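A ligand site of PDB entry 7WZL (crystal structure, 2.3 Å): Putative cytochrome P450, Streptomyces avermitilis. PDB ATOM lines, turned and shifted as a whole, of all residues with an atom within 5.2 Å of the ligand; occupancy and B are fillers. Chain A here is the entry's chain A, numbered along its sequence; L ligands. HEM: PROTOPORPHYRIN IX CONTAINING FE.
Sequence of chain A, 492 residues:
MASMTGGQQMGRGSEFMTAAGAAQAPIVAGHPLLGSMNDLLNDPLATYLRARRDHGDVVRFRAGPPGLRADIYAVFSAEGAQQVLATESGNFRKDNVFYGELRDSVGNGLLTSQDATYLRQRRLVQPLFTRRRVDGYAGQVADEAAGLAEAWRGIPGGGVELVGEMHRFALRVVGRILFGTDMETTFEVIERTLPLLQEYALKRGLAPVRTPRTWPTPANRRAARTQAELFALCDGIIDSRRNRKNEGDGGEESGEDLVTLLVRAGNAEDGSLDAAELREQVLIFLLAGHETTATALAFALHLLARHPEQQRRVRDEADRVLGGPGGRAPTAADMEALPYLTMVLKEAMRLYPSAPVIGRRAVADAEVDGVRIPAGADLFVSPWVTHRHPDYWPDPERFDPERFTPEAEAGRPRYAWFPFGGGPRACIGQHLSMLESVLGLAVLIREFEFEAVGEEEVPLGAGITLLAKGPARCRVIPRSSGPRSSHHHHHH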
ATOM      1  N   LEU A  85      -4.413   1.461  10.703  1.00  0.00           N
ATOM      2  CA  LEU A  85      -4.973   1.580   9.345  1.00  0.00           C
ATOM      3  C   LEU A  85      -4.092   0.894   8.308  1.00  0.00           C
ATOM      4  O   LEU A  85      -4.605   0.228   7.500  1.00  0.00           O
ATOM      5  CB  LEU A  85      -5.239   3.054   9.032  1.00  0.00           C
ATOM      6  CG  LEU A  85      -6.289   3.754   9.877  1.00  0.00           C
ATOM      7  CD1 LEU A  85      -6.466   5.190   9.421  1.00  0.00           C
ATOM      8  CD2 LEU A  85      -7.618   3.019   9.824  1.00  0.00           C
ATOM      9  N   LYS A  94     -13.552  -3.945  10.203  1.00  0.00           N
ATOM     10  CA  LYS A  94     -14.787  -3.132  10.301  1.00  0.00           C
ATOM     11  C   LYS A  94     -15.883  -4.036  10.860  1.00  0.00           C
ATOM     12  O   LYS A  94     -16.898  -4.212  10.197  1.00  0.00           O
ATOM     13  CB  LYS A  94     -15.111  -2.593   8.920  1.00  0.00           C
ATOM     14  CG  LYS A  94     -13.991  -1.796   8.268  1.00  0.00           C
ATOM     15  CD  LYS A  94     -14.480  -0.844   7.204  1.00  0.00           C
ATOM     16  CE  LYS A  94     -13.354  -0.208   6.420  1.00  0.00           C
ATOM     17  NZ  LYS A  94     -13.786   1.034   5.745  1.00  0.00           N
ATOM     18  N   TYR A  99     -21.088  -0.682  11.751  1.00  0.00           N
ATOM     19  CA  TYR A  99     -20.907  -1.131  10.355  1.00  0.00           C
ATOM     20  C   TYR A  99     -22.026  -2.098   9.990  1.00  0.00           C
ATOM     21  O   TYR A  99     -22.554  -1.994   8.889  1.00  0.00           O
ATOM     22  CB  TYR A  99     -19.518  -1.727  10.168  1.00  0.00           C
ATOM     23  CG  TYR A  99     -18.389  -0.726  10.179  1.00  0.00           C
ATOM     24  CD1 TYR A  99     -18.228   0.178   9.158  1.00  0.00           C
ATOM     25  CD2 TYR A  99     -17.469  -0.707  11.224  1.00  0.00           C
ATOM     26  CE1 TYR A  99     -17.180   1.100   9.158  1.00  0.00           C
ATOM     27  CE2 TYR A  99     -16.425   0.196  11.239  1.00  0.00           C
ATOM     28  CZ  TYR A  99     -16.270   1.097  10.205  1.00  0.00           C
ATOM     29  OH  TYR A  99     -15.252   1.988  10.211  1.00  0.00           O
ATOM     30  N   LEU A 110     -18.781  -0.636  -0.701  1.00  0.00           N
ATOM     31  CA  LEU A 110     -17.312  -0.609  -0.745  1.00  0.00           C
ATOM     32  C   LEU A 110     -16.802  -0.118   0.616  1.00  0.00           C
ATOM     33  O   LEU A 110     -15.807  -0.661   1.074  1.00  0.00           O
ATOM     34  CB  LEU A 110     -16.863   0.291  -1.907  1.00  0.00           C
ATOM     35  CG  LEU A 110     -15.396   0.163  -2.291  1.00  0.00           C
ATOM     36  CD1 LEU A 110     -15.162  -1.090  -3.126  1.00  0.00           C
ATOM     37  CD2 LEU A 110     -14.940   1.414  -3.027  1.00  0.00           C
ATOM     38  N   LEU A 111     -17.536   0.747   1.314  1.00  0.00           N
ATOM     39  CA  LEU A 111     -17.094   1.268   2.626  1.00  0.00           C
ATOM     40  C   LEU A 111     -17.229   0.202   3.723  1.00  0.00           C
ATOM     41  O   LEU A 111     -16.375   0.174   4.602  1.00  0.00           O
ATOM     42  CB  LEU A 111     -17.916   2.519   2.960  1.00  0.00           C
ATOM     43  CG  LEU A 111     -17.401   3.353   4.129  1.00  0.00           C
ATOM     44  CD1 LEU A 111     -17.195   4.803   3.716  1.00  0.00           C
ATOM     45  CD2 LEU A 111     -18.378   3.289   5.296  1.00  0.00           C
ATOM     46  N   TYR A 118     -15.292  -7.507  -0.640  1.00  0.00           N
ATOM     47  CA  TYR A 118     -14.666  -6.193  -0.893  1.00  0.00           C
ATOM     48  C   TYR A 118     -13.754  -6.273  -2.108  1.00  0.00           C
ATOM     49  O   TYR A 118     -13.801  -5.365  -2.912  1.00  0.00           O
ATOM     50  CB  TYR A 118     -13.856  -5.711   0.308  1.00  0.00           C
ATOM     51  CG  TYR A 118     -13.067  -4.464   0.024  1.00  0.00           C
ATOM     52  CD1 TYR A 118     -13.698  -3.242  -0.109  1.00  0.00           C
ATOM     53  CD2 TYR A 118     -11.696  -4.511  -0.186  1.00  0.00           C
ATOM     54  CE1 TYR A 118     -12.989  -2.088  -0.401  1.00  0.00           C
ATOM     55  CE2 TYR A 118     -10.969  -3.379  -0.488  1.00  0.00           C
ATOM     56  CZ  TYR A 118     -11.620  -2.167  -0.593  1.00  0.00           C
ATOM     57  OH  TYR A 118     -10.915  -1.032  -0.870  1.00  0.00           O
ATOM     58  N   ARG A 122     -13.847  -3.788  -5.182  1.00  0.00           N
ATOM     59  CA  ARG A 122     -12.689  -2.903  -5.490  1.00  0.00           C
ATOM     60  C   ARG A 122     -12.261  -3.115  -6.941  1.00  0.00           C
ATOM     61  O   ARG A 122     -12.037  -2.132  -7.635  1.00  0.00           O
ATOM     62  CB  ARG A 122     -11.554  -3.108  -4.487  1.00  0.00           C
ATOM     63  CG  ARG A 122     -10.308  -2.290  -4.750  1.00  0.00           C
ATOM     64  CD  ARG A 122     -10.441  -0.867  -4.239  1.00  0.00           C
ATOM     65  NE  ARG A 122      -9.170  -0.167  -4.334  1.00  0.00           N
ATOM     66  CZ  ARG A 122      -8.257  -0.124  -3.374  1.00  0.00           C
ATOM     67  NH1 ARG A 122      -8.461  -0.740  -2.225  1.00  0.00           N
ATOM     68  NH2 ARG A 122      -7.141   0.548  -3.566  1.00  0.00           N
ATOM     69  N   PHE A 129     -12.662   5.400 -10.545  1.00  0.00           N
ATOM     70  CA  PHE A 129     -12.103   6.438  -9.651  1.00  0.00           C
ATOM     71  C   PHE A 129     -10.658   6.736 -10.047  1.00  0.00           C
ATOM     72  O   PHE A 129      -9.877   7.154  -9.193  1.00  0.00           O
ATOM     73  CB  PHE A 129     -12.310   6.041  -8.194  1.00  0.00           C
ATOM     74  CG  PHE A 129     -13.673   6.351  -7.653  1.00  0.00           C
ATOM     75  CD1 PHE A 129     -13.973   7.623  -7.196  1.00  0.00           C
ATOM     76  CD2 PHE A 129     -14.673   5.391  -7.623  1.00  0.00           C
ATOM     77  CE1 PHE A 129     -15.235   7.921  -6.699  1.00  0.00           C
ATOM     78  CE2 PHE A 129     -15.925   5.689  -7.130  1.00  0.00           C
ATOM     79  CZ  PHE A 129     -16.213   6.956  -6.669  1.00  0.00           C
ATOM     80  N   VAL A 174     -22.207  15.941  -6.193  1.00  0.00           N
ATOM     81  CA  VAL A 174     -22.048  14.467  -6.225  1.00  0.00           C
ATOM     82  C   VAL A 174     -23.184  13.835  -7.020  1.00  0.00           C
ATOM     83  O   VAL A 174     -22.926  12.864  -7.700  1.00  0.00           O
ATOM     84  CB  VAL A 174     -21.852  13.884  -4.811  1.00  0.00           C
ATOM     85  CG1 VAL A 174     -23.151  13.660  -4.053  1.00  0.00           C
ATOM     86  CG2 VAL A 174     -21.011  12.618  -4.819  1.00  0.00           C
ATOM     87  N   ILE A 284     -23.754   4.293  -1.038  1.00  0.00           N
ATOM     88  CA  ILE A 284     -22.491   4.505  -0.291  1.00  0.00           C
ATOM     89  C   ILE A 284     -21.760   5.732  -0.841  1.00  0.00           C
ATOM     90  O   ILE A 284     -21.219   6.466  -0.042  1.00  0.00           O
ATOM     91  CB  ILE A 284     -21.633   3.216  -0.219  1.00  0.00           C
ATOM     92  CG1 ILE A 284     -21.182   2.924   1.208  1.00  0.00           C
ATOM     93  CG2 ILE A 284     -20.462   3.220  -1.184  1.00  0.00           C
ATOM     94  CD1 ILE A 284     -22.126   3.425   2.273  1.00  0.00           C
ATOM     95  N   PHE A 285     -21.812   5.971  -2.147  1.00  0.00           N
ATOM     96  CA  PHE A 285     -21.121   7.126  -2.761  1.00  0.00           C
ATOM     97  C   PHE A 285     -21.827   8.408  -2.297  1.00  0.00           C
ATOM     98  O   PHE A 285     -21.129   9.360  -1.958  1.00  0.00           O
ATOM     99  CB  PHE A 285     -21.083   6.987  -4.288  1.00  0.00           C
ATOM    100  CG  PHE A 285     -20.227   5.860  -4.828  1.00  0.00           C
ATOM    101  CD1 PHE A 285     -19.268   5.258  -4.045  1.00  0.00           C
ATOM    102  CD2 PHE A 285     -20.399   5.419  -6.127  1.00  0.00           C
ATOM    103  CE1 PHE A 285     -18.494   4.211  -4.546  1.00  0.00           C
ATOM    104  CE2 PHE A 285     -19.624   4.380  -6.623  1.00  0.00           C
ATOM    105  CZ  PHE A 285     -18.682   3.778  -5.832  1.00  0.00           C
ATOM    106  N   ALA A 288     -20.990   8.746   1.574  1.00  0.00           N
ATOM    107  CA  ALA A 288     -19.569   9.050   1.857  1.00  0.00           C
ATOM    108  C   ALA A 288     -19.092  10.361   1.239  1.00  0.00           C
ATOM    109  O   ALA A 288     -18.028  10.802   1.639  1.00  0.00           O
ATOM    110  CB  ALA A 288     -18.703   7.919   1.387  1.00  0.00           C
ATOM    111  N   GLY A 289     -19.854  10.946   0.314  1.00  0.00           N
ATOM    112  CA  GLY A 289     -19.396  12.158  -0.371  1.00  0.00           C
ATOM    113  C   GLY A 289     -20.241  13.398  -0.136  1.00  0.00           C
ATOM    114  O   GLY A 289     -19.834  14.450  -0.604  1.00  0.00           O
ATOM    115  N   THR A 292     -19.384  14.788   4.116  1.00  0.00           N
ATOM    116  CA  THR A 292     -17.904  14.911   4.191  1.00  0.00           C
ATOM    117  C   THR A 292     -17.444  16.146   3.418  1.00  0.00           C
ATOM    118  O   THR A 292     -16.763  16.985   4.000  1.00  0.00           O
ATOM    119  CB  THR A 292     -17.296  13.606   3.682  1.00  0.00           C
ATOM    120  OG1 THR A 292     -17.802  13.382   2.361  1.00  0.00           O
ATOM    121  CG2 THR A 292     -17.589  12.428   4.579  1.00  0.00           C
ATOM    122  N   THR A 293     -17.838  16.257   2.155  1.00  0.00           N
ATOM    123  CA  THR A 293     -17.405  17.394   1.319  1.00  0.00           C
ATOM    124  C   THR A 293     -18.105  18.679   1.796  1.00  0.00           C
ATOM    125  O   THR A 293     -17.441  19.709   1.804  1.00  0.00           O
ATOM    126  CB  THR A 293     -17.523  17.062  -0.167  1.00  0.00           C
ATOM    127  OG1 THR A 293     -17.255  15.660  -0.320  1.00  0.00           O
ATOM    128  CG2 THR A 293     -16.534  17.850  -1.005  1.00  0.00           C
ATOM    129  N   MET A 349      -9.337  20.916   6.765  1.00  0.00           N
ATOM    130  CA  MET A 349      -9.638  19.486   7.070  1.00  0.00           C
ATOM    131  C   MET A 349      -8.797  19.019   8.263  1.00  0.00           C
ATOM    132  O   MET A 349      -9.134  18.000   8.835  1.00  0.00           O
ATOM    133  CB  MET A 349      -9.411  18.596   5.856  1.00  0.00           C
ATOM    134  CG  MET A 349     -10.434  18.822   4.763  1.00  0.00           C
ATOM    135  SD  MET A 349     -10.218  17.691   3.375  1.00  0.00           S
ATOM    136  CE  MET A 349      -8.702  18.321   2.670  1.00  0.00           C
ATOM    137  N   PRO A 353     -11.841  17.851  10.644  1.00  0.00           N
ATOM    138  CA  PRO A 353     -11.906  16.595   9.925  1.00  0.00           C
ATOM    139  C   PRO A 353     -13.351  16.098   9.798  1.00  0.00           C
ATOM    140  O   PRO A 353     -13.998  15.910  10.792  1.00  0.00           O
ATOM    141  CB  PRO A 353     -10.984  15.653  10.712  1.00  0.00           C
ATOM    142  CG  PRO A 353     -10.962  16.212  12.095  1.00  0.00           C
ATOM    143  CD  PRO A 353     -11.135  17.699  11.911  1.00  0.00           C
ATOM    144  N   SER A 354     -13.806  15.922   8.560  1.00  0.00           N
ATOM    145  CA  SER A 354     -15.201  15.480   8.329  1.00  0.00           C
ATOM    146  C   SER A 354     -15.387  14.110   8.976  1.00  0.00           C
ATOM    147  O   SER A 354     -16.452  13.886   9.455  1.00  0.00           O
ATOM    148  CB  SER A 354     -15.568  15.530   6.887  1.00  0.00           C
ATOM    149  OG  SER A 354     -15.030  16.697   6.276  1.00  0.00           O
ATOM    150  N   ALA A 355     -14.374  13.252   8.993  1.00  0.00           N
ATOM    151  CA  ALA A 355     -14.458  11.998   9.767  1.00  0.00           C
ATOM    152  C   ALA A 355     -13.561  12.141  11.003  1.00  0.00           C
ATOM    153  O   ALA A 355     -12.387  11.803  10.906  1.00  0.00           O
ATOM    154  CB  ALA A 355     -14.065  10.804   8.945  1.00  0.00           C
ATOM    155  N   ILE A 358     -12.233   7.104  13.292  1.00  0.00           N
ATOM    156  CA  ILE A 358     -12.359   5.966  12.331  1.00  0.00           C
ATOM    157  C   ILE A 358     -12.352   4.698  13.180  1.00  0.00           C
ATOM    158  O   ILE A 358     -11.340   4.423  13.801  1.00  0.00           O
ATOM    159  CB  ILE A 358     -11.275   5.983  11.250  1.00  0.00           C
ATOM    160  CG1 ILE A 358     -11.333   7.249  10.385  1.00  0.00           C
ATOM    161  CG2 ILE A 358     -11.321   4.730  10.407  1.00  0.00           C
ATOM    162  CD1 ILE A 358     -10.019   7.631   9.759  1.00  0.00           C
ATOM    163  N   GLY A 359     -13.470   3.977  13.202  1.00  0.00           N
ATOM    164  CA  GLY A 359     -13.599   2.799  14.071  1.00  0.00           C
ATOM    165  C   GLY A 359     -13.103   1.501  13.466  1.00  0.00           C
ATOM    166  O   GLY A 359     -13.266   1.319  12.264  1.00  0.00           O
ATOM    167  N   ARG A 360     -12.521   0.646  14.306  1.00  0.00           N
ATOM    168  CA  ARG A 360     -12.043  -0.693  13.874  1.00  0.00           C
ATOM    169  C   ARG A 360     -12.268  -1.659  15.040  1.00  0.00           C
ATOM    170  O   ARG A 360     -12.659  -1.205  16.105  1.00  0.00           O
ATOM    171  CB  ARG A 360     -10.540  -0.686  13.546  1.00  0.00           C
ATOM    172  CG  ARG A 360     -10.161  -0.044  12.228  1.00  0.00           C
ATOM    173  CD  ARG A 360     -10.807  -0.722  11.041  1.00  0.00           C
ATOM    174  NE  ARG A 360     -10.266  -0.209   9.806  1.00  0.00           N
ATOM    175  CZ  ARG A 360     -10.816   0.771   9.109  1.00  0.00           C
ATOM    176  NH1 ARG A 360     -11.940   1.331   9.530  1.00  0.00           N
ATOM    177  NH2 ARG A 360     -10.267   1.180   7.982  1.00  0.00           N
ATOM    178  N   PRO A 419      -7.243  12.869   7.112  1.00  0.00           N
ATOM    179  CA  PRO A 419      -8.682  13.023   7.040  1.00  0.00           C
ATOM    180  C   PRO A 419      -9.373  12.041   6.077  1.00  0.00           C
ATOM    181  O   PRO A 419     -10.509  11.734   6.308  1.00  0.00           O
ATOM    182  CB  PRO A 419      -8.853  14.485   6.597  1.00  0.00           C
ATOM    183  CG  PRO A 419      -7.649  14.751   5.758  1.00  0.00           C
ATOM    184  CD  PRO A 419      -6.558  13.986   6.462  1.00  0.00           C
ATOM    185  N   PHE A 420      -8.654  11.548   5.075  1.00  0.00           N
ATOM    186  CA  PHE A 420      -9.211  10.578   4.094  1.00  0.00           C
ATOM    187  C   PHE A 420      -8.816   9.177   4.520  1.00  0.00           C
ATOM    188  O   PHE A 420      -8.937   8.243   3.739  1.00  0.00           O
ATOM    189  CB  PHE A 420      -8.707  10.940   2.704  1.00  0.00           C
ATOM    190  CG  PHE A 420      -9.115  12.292   2.202  1.00  0.00           C
ATOM    191  CD1 PHE A 420     -10.363  12.486   1.642  1.00  0.00           C
ATOM    192  CD2 PHE A 420      -8.247  13.369   2.271  1.00  0.00           C
ATOM    193  CE1 PHE A 420     -10.741  13.721   1.153  1.00  0.00           C
ATOM    194  CE2 PHE A 420      -8.623  14.613   1.787  1.00  0.00           C
ATOM    195  CZ  PHE A 420      -9.869  14.793   1.230  1.00  0.00           C
ATOM    196  N   GLY A 421      -8.348   9.053   5.752  1.00  0.00           N
ATOM    197  CA  GLY A 421      -7.891   7.753   6.264  1.00  0.00           C
ATOM    198  C   GLY A 421      -6.523   7.424   5.734  1.00  0.00           C
ATOM    199  O   GLY A 421      -5.731   8.358   5.518  1.00  0.00           O
ATOM    200  N   PRO A 424      -4.894   0.446   2.880  1.00  0.00           N
ATOM    201  CA  PRO A 424      -5.728  -0.219   1.882  1.00  0.00           C
ATOM    202  C   PRO A 424      -7.192   0.242   1.787  1.00  0.00           C
ATOM    203  O   PRO A 424      -7.786   0.051   0.772  1.00  0.00           O
ATOM    204  CB  PRO A 424      -5.684  -1.680   2.334  1.00  0.00           C
ATOM    205  CG  PRO A 424      -5.379  -1.619   3.813  1.00  0.00           C
ATOM    206  CD  PRO A 424      -4.421  -0.452   3.935  1.00  0.00           C
ATOM    207  N   ARG A 425      -7.722   0.836   2.866  1.00  0.00           N
ATOM    208  CA  ARG A 425      -9.136   1.275   2.901  1.00  0.00           C
ATOM    209  C   ARG A 425      -9.207   2.797   2.935  1.00  0.00           C
ATOM    210  O   ARG A 425     -10.248   3.297   3.367  1.00  0.00           O
ATOM    211  CB  ARG A 425      -9.887   0.530   4.011  1.00  0.00           C
ATOM    212  CG  ARG A 425      -9.706  -0.973   4.001  1.00  0.00           C
ATOM    213  CD  ARG A 425     -10.402  -1.633   2.824  1.00  0.00           C
ATOM    214  NE  ARG A 425     -11.807  -1.282   2.759  1.00  0.00           N
ATOM    215  CZ  ARG A 425     -12.805  -2.053   3.152  1.00  0.00           C
ATOM    216  NH1 ARG A 425     -12.558  -3.260   3.645  1.00  0.00           N
ATOM    217  NH2 ARG A 425     -14.040  -1.631   3.052  1.00  0.00           N
ATOM    218  N   ALA A 426      -8.200   3.481   2.418  1.00  0.00           N
ATOM    219  CA  ALA A 426      -8.272   4.954   2.306  1.00  0.00           C
ATOM    220  C   ALA A 426      -9.415   5.382   1.386  1.00  0.00           C
ATOM    221  O   ALA A 426      -9.857   4.581   0.561  1.00  0.00           O
ATOM    222  CB  ALA A 426      -6.956   5.475   1.806  1.00  0.00           C
ATOM    223  N   CYS A 427      -9.832   6.631   1.499  1.00  0.00           N
ATOM    224  CA  CYS A 427     -10.932   7.184   0.676  1.00  0.00           C
ATOM    225  C   CYS A 427     -10.661   7.058  -0.825  1.00  0.00           C
ATOM    226  O   CYS A 427      -9.629   7.549  -1.272  1.00  0.00           O
ATOM    227  CB  CYS A 427     -11.118   8.659   1.004  1.00  0.00           C
ATOM    228  SG  CYS A 427     -12.418   9.469   0.043  1.00  0.00           S
ATOM    229  N   ILE A 428     -11.583   6.438  -1.561  1.00  0.00           N
ATOM    230  CA  ILE A 428     -11.444   6.294  -3.037  1.00  0.00           C
ATOM    231  C   ILE A 428     -11.806   7.608  -3.726  1.00  0.00           C
ATOM    232  O   ILE A 428     -11.303   7.845  -4.837  1.00  0.00           O
ATOM    233  CB  ILE A 428     -12.254   5.081  -3.552  1.00  0.00           C
ATOM    234  CG1 ILE A 428     -11.622   4.433  -4.792  1.00  0.00           C
ATOM    235  CG2 ILE A 428     -13.715   5.429  -3.784  1.00  0.00           C
ATOM    236  CD1 ILE A 428     -12.377   3.242  -5.307  1.00  0.00           C
ATOM    237  N   GLY A 429     -12.607   8.468  -3.076  1.00  0.00           N
ATOM    238  CA  GLY A 429     -13.019   9.749  -3.660  1.00  0.00           C
ATOM    239  C   GLY A 429     -12.222  10.922  -3.150  1.00  0.00           C
ATOM    240  O   GLY A 429     -12.743  12.024  -3.170  1.00  0.00           O
ATOM    241  N   GLN A 430     -10.988  10.680  -2.691  1.00  0.00           N
ATOM    242  CA  GLN A 430     -10.136  11.760  -2.139  1.00  0.00           C
ATOM    243  C   GLN A 430      -9.863  12.811  -3.223  1.00  0.00           C
ATOM    244  O   GLN A 430     -10.090  13.986  -2.965  1.00  0.00           O
ATOM    245  CB  GLN A 430      -8.847  11.183  -1.549  1.00  0.00           C
ATOM    246  CG  GLN A 430      -7.768  12.213  -1.266  1.00  0.00           C
ATOM    247  CD  GLN A 430      -6.623  11.639  -0.465  1.00  0.00           C
ATOM    248  OE1 GLN A 430      -6.540  10.434  -0.251  1.00  0.00           O
ATOM    249  NE2 GLN A 430      -5.731  12.501  -0.021  1.00  0.00           N
ATOM    250  N   LEU A 432     -11.551  13.234  -6.060  1.00  0.00           N
ATOM    251  CA  LEU A 432     -12.856  13.836  -6.448  1.00  0.00           C
ATOM    252  C   LEU A 432     -13.225  14.948  -5.459  1.00  0.00           C
ATOM    253  O   LEU A 432     -13.625  16.014  -5.905  1.00  0.00           O
ATOM    254  CB  LEU A 432     -13.926  12.752  -6.501  1.00  0.00           C
ATOM    255  CG  LEU A 432     -15.290  13.170  -7.042  1.00  0.00           C
ATOM    256  CD1 LEU A 432     -15.133  13.865  -8.386  1.00  0.00           C
ATOM    257  CD2 LEU A 432     -16.217  11.977  -7.170  1.00  0.00           C
ATOM    258  N   SER A 433     -13.083  14.686  -4.172  1.00  0.00           N
ATOM    259  CA  SER A 433     -13.416  15.682  -3.134  1.00  0.00           C
ATOM    260  C   SER A 433     -12.551  16.932  -3.325  1.00  0.00           C
ATOM    261  O   SER A 433     -13.090  18.017  -3.219  1.00  0.00           O
ATOM    262  CB  SER A 433     -13.273  15.098  -1.760  1.00  0.00           C
ATOM    263  OG  SER A 433     -12.213  15.705  -1.060  1.00  0.00           O
ATOM    264  N   GLU A 436     -13.654  18.858  -6.403  1.00  0.00           N
ATOM    265  CA  GLU A 436     -14.913  19.583  -6.170  1.00  0.00           C
ATOM    266  C   GLU A 436     -14.694  20.750  -5.197  1.00  0.00           C
ATOM    267  O   GLU A 436     -15.357  21.764  -5.358  1.00  0.00           O
ATOM    268  CB  GLU A 436     -16.057  18.604  -5.930  1.00  0.00           C
ATOM    269  CG  GLU A 436     -16.293  18.165  -4.512  1.00  0.00           C
ATOM    270  CD  GLU A 436     -17.508  17.260  -4.446  1.00  0.00           C
ATOM    271  OE1 GLU A 436     -18.528  17.669  -3.852  1.00  0.00           O
ATOM    272  OE2 GLU A 436     -17.455  16.155  -5.024  1.00  0.00           O
HETATM  273  CHA HEM L   1     -13.579   5.966   2.581  1.00  0.00           C
HETATM  274  CHB HEM L   1     -16.230   7.784  -1.094  1.00  0.00           C
HETATM  275  CHC HEM L   1     -15.146  12.285   0.266  1.00  0.00           C
HETATM  276  CHD HEM L   1     -13.156  10.459   4.250  1.00  0.00           C
HETATM  277  C1A HEM L   1     -14.417   6.097   1.478  1.00  0.00           C
HETATM  278  C2A HEM L   1     -14.889   5.000   0.747  1.00  0.00           C
HETATM  279  C3A HEM L   1     -15.642   5.508  -0.257  1.00  0.00           C
HETATM  280  C4A HEM L   1     -15.631   6.938  -0.193  1.00  0.00           C
HETATM  281  CMA HEM L   1     -16.385   4.720  -1.301  1.00  0.00           C
HETATM  282  CAA HEM L   1     -14.566   3.558   1.040  1.00  0.00           C
HETATM  283  CBA HEM L   1     -13.217   3.248   0.352  1.00  0.00           C
HETATM  284  CGA HEM L   1     -12.800   1.773   0.491  1.00  0.00           C
HETATM  285  O1A HEM L   1     -12.994   1.113   1.543  1.00  0.00           O
HETATM  286  O2A HEM L   1     -12.214   1.194  -0.466  1.00  0.00           O
HETATM  287  C1B HEM L   1     -16.120   9.193  -1.078  1.00  0.00           C
HETATM  288  C2B HEM L   1     -16.710  10.053  -2.076  1.00  0.00           C
HETATM  289  C3B HEM L   1     -16.417  11.296  -1.652  1.00  0.00           C
HETATM  290  C4B HEM L   1     -15.599  11.163  -0.427  1.00  0.00           C
HETATM  291  CMB HEM L   1     -17.566   9.675  -3.303  1.00  0.00           C
HETATM  292  CAB HEM L   1     -16.567  12.644  -2.216  1.00  0.00           C
HETATM  293  CBB HEM L   1     -16.368  12.850  -3.483  1.00  0.00           C
HETATM  294  C1C HEM L   1     -14.549  12.226   1.516  1.00  0.00           C
HETATM  295  C2C HEM L   1     -14.081  13.328   2.240  1.00  0.00           C
HETATM  296  C3C HEM L   1     -13.534  12.801   3.369  1.00  0.00           C
HETATM  297  C4C HEM L   1     -13.641  11.366   3.335  1.00  0.00           C
HETATM  298  CMC HEM L   1     -14.152  14.793   1.943  1.00  0.00           C
HETATM  299  CAC HEM L   1     -13.012  13.733   4.392  1.00  0.00           C
HETATM  300  CBC HEM L   1     -13.040  13.390   5.644  1.00  0.00           C
HETATM  301  C1D HEM L   1     -13.098   9.081   4.123  1.00  0.00           C
HETATM  302  C2D HEM L   1     -12.441   8.215   5.123  1.00  0.00           C
HETATM  303  C3D HEM L   1     -12.590   6.964   4.651  1.00  0.00           C
HETATM  304  C4D HEM L   1     -13.271   7.087   3.341  1.00  0.00           C
HETATM  305  CMD HEM L   1     -11.783   8.486   6.465  1.00  0.00           C
HETATM  306  CAD HEM L   1     -12.035   5.716   5.328  1.00  0.00           C
HETATM  307  CBD HEM L   1     -13.035   5.086   6.286  1.00  0.00           C
HETATM  308  CGD HEM L   1     -12.374   3.908   6.958  1.00  0.00           C
HETATM  309  O1D HEM L   1     -11.198   3.643   6.701  1.00  0.00           O
HETATM  310  O2D HEM L   1     -13.011   3.147   7.721  1.00  0.00           O
HETATM  311  NA  HEM L   1     -14.839   7.278   0.848  1.00  0.00           N
HETATM  312  NB  HEM L   1     -15.489   9.899  -0.135  1.00  0.00           N
HETATM  313  NC  HEM L   1     -14.252  11.075   2.187  1.00  0.00           N
HETATM  314  ND  HEM L   1     -13.572   8.375   3.067  1.00  0.00           N
HETATM  315 FE   HEM L   1     -14.369   9.120   1.480  1.00  0.00          FE
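O of Leu 110 sits close to O1A of the ligand, 3.4 Å away. A nitrogen (NB) of the ligand sits close to the backbone carbonyl oxygen of Ala 288 (3.2 Å). Tyr 99 touches the ligand (OH to O2D, 3.5 Å). Leu 111 touches the ligand. Phe 285 touches the ligand. Gly 289 touches the ligand (CA to C3B, 3.4 Å). CB of Thr 292 touches C2C of the ligand, 3.5 Å away. Thr 293 touches the ligand (OG1 to CAB, 3.6 Å). Ser 354 touches the ligand (CB to CBC, 3.5 Å). Ala 355 touches the ligand (N to CBC, 3.6 Å). Ile 358 touches the ligand. O of Pro 419 touches CBC of the ligand (3.1 Å). Phe 420 touches the ligand. N of Gly 421 touches CMD of the ligand (3.6 Å). Ala 426 touches the ligand. CG2 of Ile 428 touches CMA of the ligand, at 3.7 Å. Gly 429 touches the ligand. Leu 432 touches the ligand. Ser 433 touches the ligand. OE2 of Glu 436 touches CBB of the ligand (3.8 Å). Hydrophobic or aromatic side chains that line the ligand: Leu 110, Leu 111, Tyr 118, Phe 285, Ala 288, Ile 358, Phe 420, Ile 428 and Leu 432. 25 residues have an atom within 4 Å of the ligand: Lys 94, Tyr 99, Leu 110, Leu 111, Tyr 118, Phe 285, Ala 288, Gly 289, Thr 292, Thr 293, Ser 354, Ala 355, Ile 358, Arg 360, Pro 419, Phe 420, Gly 421, Arg 425, Ala 426, Cys 427, Ile 428, Gly 429, Leu 432, Ser 433 and Glu 436. The nearest printed residue that does not touch the ligand is Ile 284 (4.3 Å).
N of Cys 427 sits at hydrogen-bond distance from O of Phe 420 (2.9 Å). The guanidinium group of Arg 122 is in hydrogen-bond range of the side-chain hydroxyl of Tyr 118 (2.8 Å). The guanidinium group (NH2) of Arg 425 sits at hydrogen-bond distance from the backbone carbonyl oxygen (O) of Leu 110 (2.8 Å). NH2 of Arg 425 sits at hydrogen-bond distance from O of Leu 111, 3.3 Å away. The side-chain amino group of Lys 94 is in hydrogen-bond range of the backbone carbonyl oxygen of Leu 111 (3.0 Å). The backbone carbonyl oxygen (O) of Thr 292 is in hydrogen-bond range of the side-chain hydroxyl (OG) of Ser 354 (2.9 Å). The backbone carbonyl oxygen of Gly 359 lies within hydrogen-bond range of the side-chain hydroxyl of Tyr 99. The side-chain hydroxyl (OG) of Ser 433 is in hydrogen-bond range of the backbone carbonyl oxygen (O) of Gln 430, 3.3 Å away.
SG of Cys 427 is bound to FE of the ligand. An oxygen (O2A) of the ligand sits at hydrogen-bond distance from the side-chain hydroxyl (OH) of Tyr 118, 2.6 Å away. An oxygen (O2D) of the ligand lies within salt-bridge range of the guanidinium group of Arg 360 (2.8 Å). NE of Arg 425 is in salt-bridge range of O1A of the ligand. An oxygen (O2D) of the ligand is in salt-bridge range of the side-chain amino group (NZ) of Lys 94 (3.0 Å).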
